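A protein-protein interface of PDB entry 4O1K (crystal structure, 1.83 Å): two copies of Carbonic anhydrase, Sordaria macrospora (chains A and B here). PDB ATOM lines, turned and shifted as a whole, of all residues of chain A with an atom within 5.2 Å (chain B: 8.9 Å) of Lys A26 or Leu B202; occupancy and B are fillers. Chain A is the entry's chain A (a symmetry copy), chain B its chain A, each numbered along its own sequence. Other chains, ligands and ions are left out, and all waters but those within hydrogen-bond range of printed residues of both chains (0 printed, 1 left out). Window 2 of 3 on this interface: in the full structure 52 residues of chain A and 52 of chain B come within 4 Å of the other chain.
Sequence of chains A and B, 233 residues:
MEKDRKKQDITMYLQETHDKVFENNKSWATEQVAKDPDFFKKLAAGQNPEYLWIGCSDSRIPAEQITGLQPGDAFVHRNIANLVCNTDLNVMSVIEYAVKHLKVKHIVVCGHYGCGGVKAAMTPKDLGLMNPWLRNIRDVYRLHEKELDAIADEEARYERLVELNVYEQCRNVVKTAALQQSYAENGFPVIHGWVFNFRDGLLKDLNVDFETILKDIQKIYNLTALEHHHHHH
The side-chain amide nitrogen (ND2) of Asn A25 is in hydrogen-bond range of the backbone carbonyl oxygen (O) of Ile B66, at 2.9 Å.
The backbone NH (N) of Leu B203 is in hydrogen-bond range of the side-chain amide oxygen (OD1) of Asn A25 (2.9 Å).
The side-chain amide oxygen (OE1) of Gln B65 sits at hydrogen-bond distance from the indole nitrogen (NE1) of Trp A28 (3.2 Å).
The backbone carbonyl oxygen of Gly B201 lies within hydrogen-bond range of the side-chain amide nitrogen of Asn A25 (3.0 Å).
O of Lys A26 is in hydrogen-bond range of OG1 of Thr A30 (2.6 Å).
The backbone carbonyl oxygen (O) of Trp B194 is in hydrogen-bond range of the backbone NH (N) of Gly B111, at 2.9 Å.
The backbone NH (N) of Asn B197 is in hydrogen-bond range of the backbone carbonyl oxygen (O) of Leu B202, 3.2 Å away.
N of Lys B204 sits at hydrogen-bond distance from O of Val B195.
OD1 of Asp B200 sits at hydrogen-bond distance from N of Leu B202, 3.2 Å away.
No position is printed for both chains.
CZ of Phe A22 touches NE1 of Trp B194, at 3.7 Å.
Phe A22 touches Leu B203.
Phe A22 touches Lys B204 (CE1 to C, 3.9 Å).
Phe A22 touches Asp B205 (CZ to CB, 3.5 Å).
Thr B67 touches Asn A24.
Asn A25 touches Leu B202 (OD1 to CA, 3.4 Å).
Lys A26 touches Leu B202.
Trp A28 touches Gly B201.
Hydrophobic or aromatic side chains of chain A within 4 Å of the printed part of chain B: Phe A22 and Trp A28.
Of the 20 printed residues of chain B, 9 touch a printed residue of chain A.
Of the printed residues of chain B, Asn A24 touches Thr B67 (3.3 Å).
Asn A25 touches just these residues of chain B: Ile B66 (2.9 Å), Gly B201 (3.0 Å), Leu B202 (3.4 Å) and Leu B203 (2.9 Å).
Lys A26 touches just one residue of chain B: Leu B202 (3.3 Å).
No residue of chain B comes within 4 Å of Ser A27.
Of the printed residues of chain A, Trp B194 touches Phe A22.
Asn B197 touches none of the printed residues of chain A.
Arg B199 touches none of the printed residues of chain A.
Of chain A, only Asn A25 (3.4 Å) and Lys A26 (3.3 Å) come within 4 Å of Leu B202.
Printed residues of chain A within 4 Å of Lys B204: Phe A22.
The nearest printed residue of chain A that does not touch Leu B202 is Ala A29 (5.2 Å).
The nearest printed residue of chain A that does not touch Ile B66 is Trp A28 (4.3 Å).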
ATOM      1  N   PHE A  22     -10.616 -18.149  -0.285  1.00  0.00           N
ATOM      2  CA  PHE A  22     -11.192 -16.813  -0.342  1.00  0.00           C
ATOM      3  C   PHE A  22     -10.411 -15.870  -1.267  1.00  0.00           C
ATOM      4  O   PHE A  22     -11.001 -15.019  -1.942  1.00  0.00           O
ATOM      5  CB  PHE A  22     -11.404 -16.244   1.066  1.00  0.00           C
ATOM      6  CG  PHE A  22     -12.587 -16.866   1.778  1.00  0.00           C
ATOM      7  CD1 PHE A  22     -13.853 -16.318   1.642  1.00  0.00           C
ATOM      8  CD2 PHE A  22     -12.433 -18.017   2.545  1.00  0.00           C
ATOM      9  CE1 PHE A  22     -14.955 -16.899   2.268  1.00  0.00           C
ATOM     10  CE2 PHE A  22     -13.527 -18.606   3.186  1.00  0.00           C
ATOM     11  CZ  PHE A  22     -14.789 -18.049   3.039  1.00  0.00           C
ATOM     12  N   GLU A  23      -9.093 -16.043  -1.319  1.00  0.00           N
ATOM     13  CA  GLU A  23      -8.268 -15.259  -2.227  1.00  0.00           C
ATOM     14  C   GLU A  23      -8.575 -15.664  -3.676  1.00  0.00           C
ATOM     15  O   GLU A  23      -8.688 -14.810  -4.550  1.00  0.00           O
ATOM     16  CB  GLU A  23      -6.785 -15.456  -1.894  1.00  0.00           C
ATOM     17  CG  GLU A  23      -6.478 -15.358  -0.392  1.00  0.00           C
ATOM     18  CD  GLU A  23      -5.078 -15.841  -0.032  1.00  0.00           C
ATOM     19  OE1 GLU A  23      -4.154 -15.696  -0.867  1.00  0.00           O
ATOM     20  OE2 GLU A  23      -4.904 -16.363   1.092  1.00  0.00           O
ATOM     21  N   ASN A  24      -8.736 -16.962  -3.924  1.00  0.00           N
ATOM     22  CA  ASN A  24      -9.068 -17.434  -5.265  1.00  0.00           C
ATOM     23  C   ASN A  24     -10.468 -16.981  -5.705  1.00  0.00           C
ATOM     24  O   ASN A  24     -10.719 -16.782  -6.901  1.00  0.00           O
ATOM     25  CB  ASN A  24      -8.937 -18.955  -5.344  1.00  0.00           C
ATOM     26  CG  ASN A  24      -7.494 -19.406  -5.440  1.00  0.00           C
ATOM     27  OD1 ASN A  24      -6.608 -18.611  -5.744  1.00  0.00           O
ATOM     28  ND2 ASN A  24      -7.254 -20.690  -5.199  1.00  0.00           N
ATOM     29  N   ASN A  25     -11.369 -16.822  -4.735  1.00  0.00           N
ATOM     30  CA  ASN A  25     -12.700 -16.272  -5.001  1.00  0.00           C
ATOM     31  C   ASN A  25     -12.667 -14.802  -5.439  1.00  0.00           C
ATOM     32  O   ASN A  25     -13.326 -14.430  -6.413  1.00  0.00           O
ATOM     33  CB  ASN A  25     -13.616 -16.428  -3.788  1.00  0.00           C
ATOM     34  CG  ASN A  25     -14.885 -15.593  -3.910  1.00  0.00           C
ATOM     35  OD1 ASN A  25     -15.075 -14.605  -3.185  1.00  0.00           O
ATOM     36  ND2 ASN A  25     -15.742 -15.963  -4.857  1.00  0.00           N
ATOM     37  N   LYS A  26     -11.904 -13.973  -4.726  1.00  0.00           N
ATOM     38  CA  LYS A  26     -11.747 -12.568  -5.109  1.00  0.00           C
ATOM     39  C   LYS A  26     -11.095 -12.425  -6.486  1.00  0.00           C
ATOM     40  O   LYS A  26     -11.499 -11.578  -7.292  1.00  0.00           O
ATOM     41  CB  LYS A  26     -10.932 -11.802  -4.062  1.00  0.00           C
ATOM     42  CG  LYS A  26     -11.631 -11.678  -2.713  1.00  0.00           C
ATOM     43  CD  LYS A  26     -10.722 -11.042  -1.666  1.00  0.00           C
ATOM     44  CE  LYS A  26     -11.344 -11.124  -0.284  1.00  0.00           C
ATOM     45  NZ  LYS A  26     -12.619 -10.362  -0.190  1.00  0.00           N
ATOM     46  N   SER A  27     -10.085 -13.255  -6.739  1.00  0.00           N
ATOM     47  CA  SER A  27      -9.410 -13.303  -8.032  1.00  0.00           C
ATOM     48  C   SER A  27     -10.381 -13.649  -9.149  1.00  0.00           C
ATOM     49  O   SER A  27     -10.349 -13.030 -10.213  1.00  0.00           O
ATOM     50  CB  SER A  27      -8.274 -14.322  -8.008  1.00  0.00           C
ATOM     51  OG  SER A  27      -7.075 -13.725  -7.560  1.00  0.00           O
ATOM     52  N   TRP A  28     -11.243 -14.633  -8.906  1.00  0.00           N
ATOM     53  CA  TRP A  28     -12.230 -15.035  -9.901  1.00  0.00           C
ATOM     54  C   TRP A  28     -13.255 -13.934 -10.159  1.00  0.00           C
ATOM     55  O   TRP A  28     -13.607 -13.674 -11.308  1.00  0.00           O
ATOM     56  CB  TRP A  28     -12.929 -16.336  -9.490  1.00  0.00           C
ATOM     57  CG  TRP A  28     -14.232 -16.577 -10.206  1.00  0.00           C
ATOM     58  CD1 TRP A  28     -14.414 -17.199 -11.412  1.00  0.00           C
ATOM     59  CD2 TRP A  28     -15.540 -16.211  -9.743  1.00  0.00           C
ATOM     60  NE1 TRP A  28     -15.756 -17.240 -11.724  1.00  0.00           N
ATOM     61  CE2 TRP A  28     -16.467 -16.635 -10.716  1.00  0.00           C
ATOM     62  CE3 TRP A  28     -16.016 -15.562  -8.601  1.00  0.00           C
ATOM     63  CZ2 TRP A  28     -17.844 -16.426 -10.577  1.00  0.00           C
ATOM     64  CZ3 TRP A  28     -17.380 -15.359  -8.463  1.00  0.00           C
ATOM     65  CH2 TRP A  28     -18.276 -15.785  -9.443  1.00  0.00           C
ATOM     66  N   ALA A  29     -13.732 -13.297  -9.090  1.00  0.00           N
ATOM     67  CA  ALA A  29     -14.646 -12.155  -9.209  1.00  0.00           C
ATOM     68  C   ALA A  29     -14.044 -10.993 -10.022  1.00  0.00           C
ATOM     69  O   ALA A  29     -14.729 -10.369 -10.840  1.00  0.00           O
ATOM     70  CB  ALA A  29     -15.066 -11.669  -7.833  1.00  0.00           C
ATOM     71  N   THR A  30     -12.768 -10.706  -9.779  1.00  0.00           N
ATOM     72  CA  THR A  30     -12.101  -9.569 -10.407  1.00  0.00           C
ATOM     73  C   THR A  30     -11.932  -9.776 -11.915  1.00  0.00           C
ATOM     74  O   THR A  30     -12.210  -8.876 -12.716  1.00  0.00           O
ATOM     75  CB  THR A  30     -10.721  -9.308  -9.777  1.00  0.00           C
ATOM     76  OG1 THR A  30     -10.825  -9.316  -8.350  1.00  0.00           O
ATOM     77  CG2 THR A  30     -10.187  -7.959 -10.218  1.00  0.00           C
ATOM     78  N   GLU A  31     -11.469 -10.964 -12.291  1.00  0.00           N
ATOM     79  CA  GLU A  31     -11.259 -11.300 -13.693  1.00  0.00           C
ATOM     80  C   GLU A  31     -12.586 -11.404 -14.447  1.00  0.00           C
ATOM     81  O   GLU A  31     -12.654 -11.100 -15.638  1.00  0.00           O
ATOM     82  CB  GLU A  31     -10.461 -12.608 -13.823  1.00  0.00           C
ATOM     83  CG  GLU A  31     -11.197 -13.846 -13.297  1.00  0.00           C
ATOM     84  CD  GLU A  31     -10.441 -15.153 -13.523  1.00  0.00           C
ATOM     85  OE1 GLU A  31      -9.219 -15.105 -13.794  1.00  0.00           O
ATOM     86  OE2 GLU A  31     -11.077 -16.230 -13.421  1.00  0.00           O
ATOM     87  N   GLN B  65     -16.173 -22.788  -9.808  1.00  0.00           N
ATOM     88  CA  GLN B  65     -15.934 -21.426 -10.273  1.00  0.00           C
ATOM     89  C   GLN B  65     -15.712 -20.453  -9.114  1.00  0.00           C
ATOM     90  O   GLN B  65     -14.687 -19.771  -9.055  1.00  0.00           O
ATOM     91  CB  GLN B  65     -17.117 -20.953 -11.119  1.00  0.00           C
ATOM     92  CG  GLN B  65     -17.080 -21.441 -12.536  1.00  0.00           C
ATOM     93  CD  GLN B  65     -15.783 -21.067 -13.190  1.00  0.00           C
ATOM     94  OE1 GLN B  65     -15.552 -19.895 -13.509  1.00  0.00           O
ATOM     95  NE2 GLN B  65     -14.907 -22.054 -13.371  1.00  0.00           N
ATOM     96  N   ILE B  66     -16.691 -20.390  -8.210  1.00  0.00           N
ATOM     97  CA  ILE B  66     -16.667 -19.508  -7.040  1.00  0.00           C
ATOM     98  C   ILE B  66     -15.383 -19.624  -6.231  1.00  0.00           C
ATOM     99  O   ILE B  66     -14.902 -18.633  -5.661  1.00  0.00           O
ATOM    100  CB  ILE B  66     -17.813 -19.843  -6.042  1.00  0.00           C
ATOM    101  CG1 ILE B  66     -19.180 -19.932  -6.716  1.00  0.00           C
ATOM    102  CG2 ILE B  66     -17.858 -18.834  -4.904  1.00  0.00           C
ATOM    103  CD1 ILE B  66     -20.303 -20.385  -5.752  1.00  0.00           C
ATOM    104  N   THR B  67     -14.840 -20.838  -6.154  1.00  0.00           N
ATOM    105  CA  THR B  67     -13.768 -21.112  -5.198  1.00  0.00           C
ATOM    106  C   THR B  67     -12.395 -21.249  -5.821  1.00  0.00           C
ATOM    107  O   THR B  67     -11.392 -21.186  -5.105  1.00  0.00           O
ATOM    108  CB  THR B  67     -14.035 -22.409  -4.448  1.00  0.00           C
ATOM    109  OG1 THR B  67     -14.181 -23.477  -5.402  1.00  0.00           O
ATOM    110  CG2 THR B  67     -15.292 -22.269  -3.637  1.00  0.00           C
ATOM    111  N   GLY B  68     -12.357 -21.464  -7.134  1.00  0.00           N
ATOM    112  CA  GLY B  68     -11.110 -21.678  -7.853  1.00  0.00           C
ATOM    113  C   GLY B  68     -10.577 -23.090  -7.680  1.00  0.00           C
ATOM    114  O   GLY B  68      -9.418 -23.370  -8.010  1.00  0.00           O
ATOM    115  N   CYS B 110     -22.848 -24.256   1.694  1.00  0.00           N
ATOM    116  CA  CYS B 110     -22.820 -22.916   1.120  1.00  0.00           C
ATOM    117  C   CYS B 110     -24.223 -22.475   0.786  1.00  0.00           C
ATOM    118  O   CYS B 110     -24.886 -23.091  -0.067  1.00  0.00           O
ATOM    119  CB  CYS B 110     -21.977 -22.903  -0.151  1.00  0.00           C
ATOM    120  SG  CYS B 110     -21.634 -21.201  -0.735  1.00  0.00           S
ATOM    121  N   GLY B 111     -24.700 -21.434   1.458  1.00  0.00           N
ATOM    122  CA  GLY B 111     -25.987 -20.886   1.068  1.00  0.00           C
ATOM    123  C   GLY B 111     -25.735 -19.728   0.122  1.00  0.00           C
ATOM    124  O   GLY B 111     -24.587 -19.466  -0.249  1.00  0.00           O
ATOM    125  N   HIS B 112     -26.795 -19.026  -0.265  1.00  0.00           N
ATOM    126  CA  HIS B 112     -26.586 -17.870  -1.139  1.00  0.00           C
ATOM    127  C   HIS B 112     -27.710 -16.877  -0.957  1.00  0.00           C
ATOM    128  O   HIS B 112     -28.864 -17.266  -0.728  1.00  0.00           O
ATOM    129  CB  HIS B 112     -26.399 -18.295  -2.606  1.00  0.00           C
ATOM    130  CG  HIS B 112     -27.621 -18.900  -3.225  1.00  0.00           C
ATOM    131  ND1 HIS B 112     -28.255 -18.342  -4.315  1.00  0.00           N
ATOM    132  CD2 HIS B 112     -28.338 -20.001  -2.892  1.00  0.00           C
ATOM    133  CE1 HIS B 112     -29.329 -19.060  -4.610  1.00  0.00           C
ATOM    134  NE2 HIS B 112     -29.389 -20.078  -3.774  1.00  0.00           N
ATOM    135  N   TYR B 113     -27.372 -15.588  -0.995  1.00  0.00           N
ATOM    136  CA  TYR B 113     -28.412 -14.572  -0.816  1.00  0.00           C
ATOM    137  C   TYR B 113     -29.298 -14.569  -2.033  1.00  0.00           C
ATOM    138  O   TYR B 113     -28.836 -14.855  -3.150  1.00  0.00           O
ATOM    139  CB  TYR B 113     -27.816 -13.172  -0.592  1.00  0.00           C
ATOM    140  CG  TYR B 113     -27.008 -13.079   0.685  1.00  0.00           C
ATOM    141  CD1 TYR B 113     -27.595 -13.322   1.921  1.00  0.00           C
ATOM    142  CD2 TYR B 113     -25.666 -12.750   0.660  1.00  0.00           C
ATOM    143  CE1 TYR B 113     -26.858 -13.250   3.093  1.00  0.00           C
ATOM    144  CE2 TYR B 113     -24.924 -12.664   1.833  1.00  0.00           C
ATOM    145  CZ  TYR B 113     -25.529 -12.919   3.045  1.00  0.00           C
ATOM    146  OH  TYR B 113     -24.801 -12.852   4.215  1.00  0.00           O
ATOM    147  N   TRP B 194     -20.630 -21.110   4.606  1.00  0.00           N
ATOM    148  CA  TRP B 194     -20.312 -19.942   3.783  1.00  0.00           C
ATOM    149  C   TRP B 194     -21.567 -19.478   3.081  1.00  0.00           C
ATOM    150  O   TRP B 194     -22.572 -20.214   3.024  1.00  0.00           O
ATOM    151  CB  TRP B 194     -19.252 -20.312   2.748  1.00  0.00           C
ATOM    152  CG  TRP B 194     -17.892 -20.734   3.298  1.00  0.00           C
ATOM    153  CD1 TRP B 194     -17.399 -20.533   4.567  1.00  0.00           C
ATOM    154  CD2 TRP B 194     -16.860 -21.432   2.575  1.00  0.00           C
ATOM    155  NE1 TRP B 194     -16.110 -21.056   4.661  1.00  0.00           N
ATOM    156  CE2 TRP B 194     -15.770 -21.621   3.457  1.00  0.00           C
ATOM    157  CE3 TRP B 194     -16.755 -21.921   1.263  1.00  0.00           C
ATOM    158  CZ2 TRP B 194     -14.580 -22.267   3.060  1.00  0.00           C
ATOM    159  CZ3 TRP B 194     -15.572 -22.566   0.874  1.00  0.00           C
ATOM    160  CH2 TRP B 194     -14.512 -22.740   1.773  1.00  0.00           C
ATOM    161  N   VAL B 195     -21.549 -18.246   2.574  1.00  0.00           N
ATOM    162  CA  VAL B 195     -22.702 -17.739   1.851  1.00  0.00           C
ATOM    163  C   VAL B 195     -22.176 -16.967   0.659  1.00  0.00           C
ATOM    164  O   VAL B 195     -21.285 -16.130   0.824  1.00  0.00           O
ATOM    165  CB  VAL B 195     -23.574 -16.801   2.706  1.00  0.00           C
ATOM    166  CG1 VAL B 195     -24.782 -16.338   1.890  1.00  0.00           C
ATOM    167  CG2 VAL B 195     -24.066 -17.502   3.940  1.00  0.00           C
ATOM    168  N   PHE B 196     -22.695 -17.277  -0.531  1.00  0.00           N
ATOM    169  CA  PHE B 196     -22.310 -16.604  -1.768  1.00  0.00           C
ATOM    170  C   PHE B 196     -23.260 -15.459  -2.043  1.00  0.00           C
ATOM    171  O   PHE B 196     -24.465 -15.544  -1.729  1.00  0.00           O
ATOM    172  CB  PHE B 196     -22.313 -17.601  -2.940  1.00  0.00           C
ATOM    173  CG  PHE B 196     -21.992 -16.986  -4.258  1.00  0.00           C
ATOM    174  CD1 PHE B 196     -20.697 -16.572  -4.553  1.00  0.00           C
ATOM    175  CD2 PHE B 196     -22.981 -16.836  -5.223  1.00  0.00           C
ATOM    176  CE1 PHE B 196     -20.397 -16.002  -5.790  1.00  0.00           C
ATOM    177  CE2 PHE B 196     -22.689 -16.258  -6.460  1.00  0.00           C
ATOM    178  CZ  PHE B 196     -21.398 -15.839  -6.738  1.00  0.00           C
ATOM    179  N   ASN B 197     -22.723 -14.390  -2.636  1.00  0.00           N
ATOM    180  CA  ASN B 197     -23.476 -13.172  -2.856  1.00  0.00           C
ATOM    181  C   ASN B 197     -23.390 -12.881  -4.353  1.00  0.00           C
ATOM    182  O   ASN B 197     -22.314 -12.484  -4.863  1.00  0.00           O
ATOM    183  CB  ASN B 197     -22.835 -12.010  -2.067  1.00  0.00           C
ATOM    184  CG  ASN B 197     -23.704 -10.758  -2.042  1.00  0.00           C
ATOM    185  OD1 ASN B 197     -24.694 -10.647  -2.768  1.00  0.00           O
ATOM    186  ND2 ASN B 197     -23.329  -9.806  -1.205  1.00  0.00           N
ATOM    187  N   PHE B 198     -24.501 -13.077  -5.057  1.00  0.00           N
ATOM    188  CA  PHE B 198     -24.557 -12.935  -6.507  1.00  0.00           C
ATOM    189  C   PHE B 198     -24.338 -11.486  -6.949  1.00  0.00           C
ATOM    190  O   PHE B 198     -24.109 -11.226  -8.134  1.00  0.00           O
ATOM    191  CB  PHE B 198     -25.924 -13.406  -7.008  1.00  0.00           C
ATOM    192  CG  PHE B 198     -27.059 -12.540  -6.531  1.00  0.00           C
ATOM    193  CD1 PHE B 198     -27.716 -12.824  -5.344  1.00  0.00           C
ATOM    194  CD2 PHE B 198     -27.456 -11.426  -7.260  1.00  0.00           C
ATOM    195  CE1 PHE B 198     -28.756 -12.021  -4.896  1.00  0.00           C
ATOM    196  CE2 PHE B 198     -28.495 -10.613  -6.821  1.00  0.00           C
ATOM    197  CZ  PHE B 198     -29.146 -10.913  -5.637  1.00  0.00           C
ATOM    198  N   ARG B 199     -24.446 -10.551  -6.005  1.00  0.00           N
ATOM    199  CA  ARG B 199     -24.337  -9.125  -6.303  1.00  0.00           C
ATOM    200  C   ARG B 199     -22.909  -8.662  -6.540  1.00  0.00           C
ATOM    201  O   ARG B 199     -22.682  -7.732  -7.327  1.00  0.00           O
ATOM    202  CB  ARG B 199     -24.952  -8.305  -5.170  1.00  0.00           C
ATOM    203  CG  ARG B 199     -26.450  -8.089  -5.322  1.00  0.00           C
ATOM    204  CD  ARG B 199     -27.188  -8.268  -4.012  1.00  0.00           C
ATOM    205  NE  ARG B 199     -28.476  -7.582  -4.036  1.00  0.00           N
ATOM    206  CZ  ARG B 199     -29.506  -7.885  -3.250  1.00  0.00           C
ATOM    207  NH1 ARG B 199     -30.638  -7.196  -3.342  1.00  0.00           N
ATOM    208  NH2 ARG B 199     -29.408  -8.881  -2.372  1.00  0.00           N
ATOM    209  N   ASP B 200     -21.955  -9.279  -5.839  1.00  0.00           N
ATOM    210  CA  ASP B 200     -20.544  -8.883  -5.952  1.00  0.00           C
ATOM    211  C   ASP B 200     -19.636 -10.080  -6.200  1.00  0.00           C
ATOM    212  O   ASP B 200     -18.424  -9.931  -6.366  1.00  0.00           O
ATOM    213  CB  ASP B 200     -20.066  -8.075  -4.737  1.00  0.00           C
ATOM    214  CG  ASP B 200     -20.437  -8.717  -3.399  1.00  0.00           C
ATOM    215  OD1 ASP B 200     -20.610  -9.963  -3.335  1.00  0.00           O
ATOM    216  OD2 ASP B 200     -20.528  -7.964  -2.396  1.00  0.00           O
ATOM    217  N   GLY B 201     -20.231 -11.265  -6.205  1.00  0.00           N
ATOM    218  CA  GLY B 201     -19.512 -12.491  -6.508  1.00  0.00           C
ATOM    219  C   GLY B 201     -18.637 -13.014  -5.385  1.00  0.00           C
ATOM    220  O   GLY B 201     -17.852 -13.947  -5.592  1.00  0.00           O
ATOM    221  N   LEU B 202     -18.799 -12.456  -4.191  1.00  0.00           N
ATOM    222  CA  LEU B 202     -17.892 -12.775  -3.098  1.00  0.00           C
ATOM    223  C   LEU B 202     -18.437 -13.867  -2.205  1.00  0.00           C
ATOM    224  O   LEU B 202     -19.651 -13.919  -1.939  1.00  0.00           O
ATOM    225  CB  LEU B 202     -17.627 -11.549  -2.246  1.00  0.00           C
ATOM    226  CG  LEU B 202     -16.433 -10.686  -2.623  1.00  0.00           C
ATOM    227  CD1 LEU B 202     -16.881  -9.477  -3.422  1.00  0.00           C
ATOM    228  CD2 LEU B 202     -15.712 -10.244  -1.368  1.00  0.00           C
ATOM    229  N   LEU B 203     -17.539 -14.737  -1.746  1.00  0.00           N
ATOM    230  CA  LEU B 203     -17.898 -15.756  -0.761  1.00  0.00           C
ATOM    231  C   LEU B 203     -17.669 -15.131   0.580  1.00  0.00           C
ATOM    232  O   LEU B 203     -16.672 -14.424   0.778  1.00  0.00           O
ATOM    233  CB  LEU B 203     -16.977 -16.962  -0.845  1.00  0.00           C
ATOM    234  CG  LEU B 203     -17.347 -18.291  -1.461  1.00  0.00           C
ATOM    235  CD1 LEU B 203     -16.316 -19.326  -1.022  1.00  0.00           C
ATOM    236  CD2 LEU B 203     -18.749 -18.721  -1.088  1.00  0.00           C
ATOM    237  N   LYS B 204     -18.565 -15.396   1.523  1.00  0.00           N
ATOM    238  CA  LYS B 204     -18.390 -14.871   2.868  1.00  0.00           C
ATOM    239  C   LYS B 204     -18.373 -16.045   3.824  1.00  0.00           C
ATOM    240  O   LYS B 204     -19.141 -16.983   3.657  1.00  0.00           O
ATOM    241  CB  LYS B 204     -19.546 -13.928   3.196  1.00  0.00           C
ATOM    242  CG  LYS B 204     -19.661 -13.502   4.655  1.00  0.00           C
ATOM    243  CD  LYS B 204     -20.843 -12.529   4.829  1.00  0.00           C
ATOM    244  CE  LYS B 204     -21.547 -12.695   6.177  1.00  0.00           C
ATOM    245  NZ  LYS B 204     -20.643 -12.601   7.373  1.00  0.00           N
ATOM    246  N   ASP B 205     -17.486 -15.988   4.806  1.00  0.00           N
ATOM    247  CA  ASP B 205     -17.405 -17.025   5.821  1.00  0.00           C
ATOM    248  C   ASP B 205     -18.292 -16.600   7.004  1.00  0.00           C
ATOM    249  O   ASP B 205     -18.143 -15.510   7.536  1.00  0.00           O
ATOM    250  CB  ASP B 205     -15.946 -17.168   6.266  1.00  0.00           C
ATOM    251  CG  ASP B 205     -15.720 -18.371   7.166  1.00  0.00           C
ATOM    252  OD1 ASP B 205     -16.709 -19.045   7.521  1.00  0.00           O
ATOM    253  OD2 ASP B 205     -14.549 -18.625   7.539  1.00  0.00           O
